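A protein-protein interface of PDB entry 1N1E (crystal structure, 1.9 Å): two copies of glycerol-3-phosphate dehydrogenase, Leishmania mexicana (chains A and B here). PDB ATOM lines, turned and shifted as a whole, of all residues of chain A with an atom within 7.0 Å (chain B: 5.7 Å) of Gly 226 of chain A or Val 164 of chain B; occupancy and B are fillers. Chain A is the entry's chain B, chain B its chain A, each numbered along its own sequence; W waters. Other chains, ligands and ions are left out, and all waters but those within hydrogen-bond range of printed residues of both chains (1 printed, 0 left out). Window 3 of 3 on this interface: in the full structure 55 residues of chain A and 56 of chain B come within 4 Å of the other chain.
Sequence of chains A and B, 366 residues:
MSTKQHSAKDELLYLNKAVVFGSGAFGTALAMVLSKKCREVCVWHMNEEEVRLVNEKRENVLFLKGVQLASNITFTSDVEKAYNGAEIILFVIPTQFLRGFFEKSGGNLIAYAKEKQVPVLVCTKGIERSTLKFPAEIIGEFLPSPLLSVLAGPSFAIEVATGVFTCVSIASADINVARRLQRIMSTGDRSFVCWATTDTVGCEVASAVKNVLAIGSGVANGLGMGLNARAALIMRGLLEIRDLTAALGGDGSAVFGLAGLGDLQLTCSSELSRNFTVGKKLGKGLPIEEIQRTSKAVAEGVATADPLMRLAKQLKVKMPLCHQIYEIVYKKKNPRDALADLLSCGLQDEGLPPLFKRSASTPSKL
Met 225 of chain A touches Phe 165 of chain B (CE to CB, 3.6 Å). Glu 159 of chain B touches Gly 226 of chain A. N of Gly 226 of chain A touches CG1 of Val 164 of chain B, at 3.6 Å. Val 160 of chain B touches Asn 228 of chain A (CG2 to ND2, 3.8 Å). Asn 228 of chain A touches Phe 165 of chain B (CB to O, 3.6 Å).
Water W1 lies within hydrogen-bond range of OE1 of Glu 159 of chain B (2.7 Å), O of Phe 165 of chain B (2.7 Å), N of Gly 226 of chain A (3.0 Å) and N of Ala 229 of chain A (3.0 Å).
The backbone NH (N) of Leu 227 of chain A is in hydrogen-bond range of the side-chain carboxylate (OE2) of Glu 159 of chain B, at 2.8 Å. OE1 of Glu 159 of chain B is in hydrogen-bond range of N of Asn 228 of chain A, 2.9 Å away. N of Ala 229 of chain A is in hydrogen-bond range of O of Phe 165 of chain B (3.4 Å). The side-chain amide nitrogen (ND2) of Asn 228 of chain A lies within hydrogen-bond range of the side-chain hydroxyl (OG1) of Thr 166 of chain B.
The backbone carbonyl oxygen (O) of Glu 159 of chain B is in hydrogen-bond range of the side-chain hydroxyl (OG1) of Thr 162 of chain B (3.5 Å). N of Val 164 of chain B lies within hydrogen-bond range of O of Glu 159 of chain B (2.9 Å). OG1 of Thr 166 of chain B lies within hydrogen-bond range of O of Val 164 of chain B (2.9 Å). The backbone carbonyl oxygen (O) of Ser 191 of chain B sits at hydrogen-bond distance from the backbone NH (N) of Thr 166 of chain B, 2.9 Å away. The backbone NH of Met 225 of chain A is in hydrogen-bond range of the backbone carbonyl oxygen of Ala 220 of chain A (3.0 Å).
No position is printed for both chains.
Of the 11 printed residues of chain A, 5 touch a printed residue of chain B. Hydrophobic or aromatic side chains of chain A within 4 Å of the printed part of chain B: Met 225, Leu 227 and Ala 229. Hydrophobic or aromatic side chains of chain B within 4 Å of the printed part of chain A: Val 160, Val 164 and Phe 165. Among the printed residues, 9 pairs touch across the chains.
Of chain B, only Glu 159 (3.5 Å) and Val 164 (3.6 Å) come within 4 Å of Gly 226 of chain A. Of the printed residues of chain B, Leu 227 of chain A touches Glu 159. Of the printed residues of chain B, Ala 229 of chain A touches Phe 165. Of the printed residues of chain A, Val 164 of chain B touches Gly 226 (3.6 Å). Of the printed residues of chain A, Thr 166 of chain B touches Asn 228.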
ATOM      1  N   SER A 217      31.283  29.163 -27.274  1.00  0.00           N
ATOM      2  CA  SER A 217      30.694  28.109 -26.462  1.00  0.00           C
ATOM      3  C   SER A 217      31.023  28.339 -24.988  1.00  0.00           C
ATOM      4  O   SER A 217      30.153  28.211 -24.126  1.00  0.00           O
ATOM      5  CB  SER A 217      31.126  26.714 -26.927  1.00  0.00           C
ATOM      6  OG  SER A 217      30.466  25.717 -26.139  1.00  0.00           O
ATOM      7  N   ALA A 220      28.865  31.088 -23.579  1.00  0.00           N
ATOM      8  CA  ALA A 220      27.557  30.533 -23.234  1.00  0.00           C
ATOM      9  C   ALA A 220      27.576  29.868 -21.869  1.00  0.00           C
ATOM     10  O   ALA A 220      26.681  30.107 -21.043  1.00  0.00           O
ATOM     11  CB  ALA A 220      27.086  29.536 -24.298  1.00  0.00           C
ATOM     12  N   ASN A 221      28.598  29.053 -21.626  1.00  0.00           N
ATOM     13  CA  ASN A 221      28.781  28.359 -20.353  1.00  0.00           C
ATOM     14  C   ASN A 221      28.944  29.359 -19.199  1.00  0.00           C
ATOM     15  O   ASN A 221      28.333  29.198 -18.150  1.00  0.00           O
ATOM     16  CB  ASN A 221      29.994  27.423 -20.434  1.00  0.00           C
ATOM     17  CG  ASN A 221      30.250  26.643 -19.128  1.00  0.00           C
ATOM     18  OD1 ASN A 221      31.205  26.925 -18.412  1.00  0.00           O
ATOM     19  ND2 ASN A 221      29.420  25.654 -18.843  1.00  0.00           N
ATOM     20  N   GLY A 224      25.883  30.984 -17.876  1.00  0.00           N
ATOM     21  CA  GLY A 224      24.926  30.108 -17.207  1.00  0.00           C
ATOM     22  C   GLY A 224      23.983  29.351 -18.144  1.00  0.00           C
ATOM     23  O   GLY A 224      23.021  28.727 -17.693  1.00  0.00           O
ATOM     24  N   MET A 225      24.247  29.408 -19.447  1.00  0.00           N
ATOM     25  CA  MET A 225      23.472  28.639 -20.416  1.00  0.00           C
ATOM     26  C   MET A 225      23.915  27.172 -20.338  1.00  0.00           C
ATOM     27  O   MET A 225      24.945  26.848 -19.746  1.00  0.00           O
ATOM     28  CB  MET A 225      23.640  29.231 -21.809  1.00  0.00           C
ATOM     29  CG  MET A 225      23.390  30.758 -21.841  1.00  0.00           C
ATOM     30  SD  MET A 225      23.738  31.539 -23.428  1.00  0.00           S
ATOM     31  CE  MET A 225      22.344  31.025 -24.333  1.00  0.00           C
ATOM     32  N   GLY A 226      23.130  26.283 -20.929  1.00  0.00           N
ATOM     33  CA  GLY A 226      23.322  24.862 -20.735  1.00  0.00           C
ATOM     34  C   GLY A 226      23.769  24.117 -21.975  1.00  0.00           C
ATOM     35  O   GLY A 226      24.285  24.690 -22.932  1.00  0.00           O
ATOM     36  N   LEU A 227      23.560  22.811 -21.937  1.00  0.00           N
ATOM     37  CA  LEU A 227      23.988  21.924 -23.000  1.00  0.00           C
ATOM     38  C   LEU A 227      23.144  22.060 -24.268  1.00  0.00           C
ATOM     39  O   LEU A 227      23.662  21.870 -25.374  1.00  0.00           O
ATOM     40  CB  LEU A 227      23.990  20.484 -22.510  1.00  0.00           C
ATOM     41  CG  LEU A 227      24.917  20.195 -21.329  1.00  0.00           C
ATOM     42  CD1 LEU A 227      24.800  18.749 -20.967  1.00  0.00           C
ATOM     43  CD2 LEU A 227      26.379  20.552 -21.617  1.00  0.00           C
ATOM     44  N   ASN A 228      21.863  22.394 -24.115  1.00  0.00           N
ATOM     45  CA  ASN A 228      20.997  22.619 -25.263  1.00  0.00           C
ATOM     46  C   ASN A 228      21.532  23.806 -26.079  1.00  0.00           C
ATOM     47  O   ASN A 228      21.611  23.736 -27.309  1.00  0.00           O
ATOM     48  CB  ASN A 228      19.532  22.861 -24.846  1.00  0.00           C
ATOM     49  CG  ASN A 228      18.874  21.640 -24.217  1.00  0.00           C
ATOM     50  OD1 ASN A 228      19.458  20.542 -24.164  1.00  0.00           O
ATOM     51  ND2 ASN A 228      17.626  21.816 -23.756  1.00  0.00           N
ATOM     52  N   ALA A 229      21.930  24.872 -25.390  1.00  0.00           N
ATOM     53  CA  ALA A 229      22.478  26.058 -26.043  1.00  0.00           C
ATOM     54  C   ALA A 229      23.792  25.743 -26.761  1.00  0.00           C
ATOM     55  O   ALA A 229      24.018  26.199 -27.867  1.00  0.00           O
ATOM     56  CB  ALA A 229      22.718  27.180 -25.032  1.00  0.00           C
ATOM     57  N   ARG A 230      24.648  24.975 -26.104  1.00  0.00           N
ATOM     58  CA  ARG A 230      25.917  24.554 -26.680  1.00  0.00           C
ATOM     59  C   ARG A 230      25.691  23.828 -28.003  1.00  0.00           C
ATOM     60  O   ARG A 230      26.344  24.119 -28.998  1.00  0.00           O
ATOM     61  CB  ARG A 230      26.642  23.638 -25.696  1.00  0.00           C
ATOM     62  CG  ARG A 230      27.946  23.041 -26.202  1.00  0.00           C
ATOM     63  CD  ARG A 230      28.591  22.148 -25.194  1.00  0.00           C
ATOM     64  NE  ARG A 230      28.935  22.884 -23.995  1.00  0.00           N
ATOM     65  CZ  ARG A 230      29.409  22.326 -22.884  1.00  0.00           C
ATOM     66  NH1 ARG A 230      29.614  21.016 -22.812  1.00  0.00           N
ATOM     67  NH2 ARG A 230      29.693  23.091 -21.845  1.00  0.00           N
ATOM     68  N   ALA A 231      24.744  22.900 -28.005  1.00  0.00           N
ATOM     69  CA  ALA A 231      24.431  22.098 -29.184  1.00  0.00           C
ATOM     70  C   ALA A 231      23.956  22.999 -30.326  1.00  0.00           C
ATOM     71  O   ALA A 231      24.340  22.808 -31.479  1.00  0.00           O
ATOM     72  CB  ALA A 231      23.367  21.069 -28.841  1.00  0.00           C
ATOM     73  N   ILE B 158      15.197  18.732 -18.593  1.00  0.00           N
ATOM     74  CA  ILE B 158      15.435  19.576 -17.431  1.00  0.00           C
ATOM     75  C   ILE B 158      15.715  21.036 -17.818  1.00  0.00           C
ATOM     76  O   ILE B 158      15.181  21.945 -17.189  1.00  0.00           O
ATOM     77  CB  ILE B 158      16.545  18.982 -16.523  1.00  0.00           C
ATOM     78  CG1 ILE B 158      16.520  19.663 -15.153  1.00  0.00           C
ATOM     79  CG2 ILE B 158      17.934  19.067 -17.186  1.00  0.00           C
ATOM     80  CD1 ILE B 158      15.331  19.186 -14.292  1.00  0.00           C
ATOM     81  N   GLU B 159      16.516  21.252 -18.858  1.00  0.00           N
ATOM     82  CA  GLU B 159      16.793  22.604 -19.365  1.00  0.00           C
ATOM     83  C   GLU B 159      15.555  23.252 -19.984  1.00  0.00           C
ATOM     84  O   GLU B 159      15.262  24.414 -19.701  1.00  0.00           O
ATOM     85  CB  GLU B 159      17.953  22.575 -20.367  1.00  0.00           C
ATOM     86  CG  GLU B 159      19.289  22.347 -19.685  1.00  0.00           C
ATOM     87  CD  GLU B 159      20.467  22.401 -20.630  1.00  0.00           C
ATOM     88  OE1 GLU B 159      20.324  22.933 -21.766  1.00  0.00           O
ATOM     89  OE2 GLU B 159      21.546  21.897 -20.228  1.00  0.00           O
ATOM     90  N   VAL B 160      14.806  22.497 -20.789  1.00  0.00           N
ATOM     91  CA  VAL B 160      13.554  22.982 -21.346  1.00  0.00           C
ATOM     92  C   VAL B 160      12.548  23.367 -20.255  1.00  0.00           C
ATOM     93  O   VAL B 160      11.954  24.436 -20.314  1.00  0.00           O
ATOM     94  CB  VAL B 160      12.913  21.949 -22.318  1.00  0.00           C
ATOM     95  CG1 VAL B 160      11.501  22.380 -22.741  1.00  0.00           C
ATOM     96  CG2 VAL B 160      13.789  21.779 -23.552  1.00  0.00           C
ATOM     97  N   THR B 162      12.934  24.249 -17.218  1.00  0.00           N
ATOM     98  CA  THR B 162      13.339  25.382 -16.372  1.00  0.00           C
ATOM     99  C   THR B 162      13.672  26.623 -17.178  1.00  0.00           C
ATOM    100  O   THR B 162      14.118  27.612 -16.616  1.00  0.00           O
ATOM    101  CB  THR B 162      14.534  25.011 -15.470  1.00  0.00           C
ATOM    102  OG1 THR B 162      15.624  24.508 -16.264  1.00  0.00           O
ATOM    103  CG2 THR B 162      14.172  23.872 -14.531  1.00  0.00           C
ATOM    104  N   GLY B 163      13.448  26.588 -18.490  1.00  0.00           N
ATOM    105  CA  GLY B 163      13.585  27.774 -19.319  1.00  0.00           C
ATOM    106  C   GLY B 163      15.016  28.157 -19.676  1.00  0.00           C
ATOM    107  O   GLY B 163      15.293  29.306 -19.976  1.00  0.00           O
ATOM    108  N   VAL B 164      15.930  27.201 -19.638  1.00  0.00           N
ATOM    109  CA  VAL B 164      17.292  27.414 -20.110  1.00  0.00           C
ATOM    110  C   VAL B 164      17.289  27.349 -21.659  1.00  0.00           C
ATOM    111  O   VAL B 164      16.642  26.468 -22.259  1.00  0.00           O
ATOM    112  CB  VAL B 164      18.254  26.375 -19.489  1.00  0.00           C
ATOM    113  CG1 VAL B 164      19.698  26.684 -19.850  1.00  0.00           C
ATOM    114  CG2 VAL B 164      18.104  26.324 -17.952  1.00  0.00           C
ATOM    115  N   PHE B 165      18.026  28.263 -22.287  1.00  0.00           N
ATOM    116  CA  PHE B 165      17.990  28.480 -23.729  1.00  0.00           C
ATOM    117  C   PHE B 165      18.069  27.182 -24.534  1.00  0.00           C
ATOM    118  O   PHE B 165      19.016  26.414 -24.393  1.00  0.00           O
ATOM    119  CB  PHE B 165      19.128  29.395 -24.173  1.00  0.00           C
ATOM    120  CG  PHE B 165      19.076  29.737 -25.631  1.00  0.00           C
ATOM    121  CD1 PHE B 165      18.223  30.734 -26.088  1.00  0.00           C
ATOM    122  CD2 PHE B 165      19.839  29.042 -26.550  1.00  0.00           C
ATOM    123  CE1 PHE B 165      18.157  31.047 -27.453  1.00  0.00           C
ATOM    124  CE2 PHE B 165      19.779  29.350 -27.914  1.00  0.00           C
ATOM    125  CZ  PHE B 165      18.938  30.352 -28.362  1.00  0.00           C
ATOM    126  N   THR B 166      17.067  26.964 -25.377  1.00  0.00           N
ATOM    127  CA  THR B 166      16.948  25.754 -26.181  1.00  0.00           C
ATOM    128  C   THR B 166      16.468  26.130 -27.583  1.00  0.00           C
ATOM    129  O   THR B 166      15.586  26.974 -27.724  1.00  0.00           O
ATOM    130  CB  THR B 166      15.948  24.800 -25.533  1.00  0.00           C
ATOM    131  OG1 THR B 166      16.423  24.378 -24.240  1.00  0.00           O
ATOM    132  CG2 THR B 166      15.783  23.515 -26.372  1.00  0.00           C
ATOM    133  N   SER B 191      13.685  31.896 -24.495  1.00  0.00           N
ATOM    134  CA  SER B 191      14.196  30.709 -23.822  1.00  0.00           C
ATOM    135  C   SER B 191      14.019  29.441 -24.670  1.00  0.00           C
ATOM    136  O   SER B 191      14.777  28.487 -24.527  1.00  0.00           O
ATOM    137  CB  SER B 191      13.480  30.540 -22.489  1.00  0.00           C
ATOM    138  OG  SER B 191      12.123  30.209 -22.681  1.00  0.00           O
HETATM  139  O   HOH W   1      20.871  25.438 -22.656  1.00  0.00           O
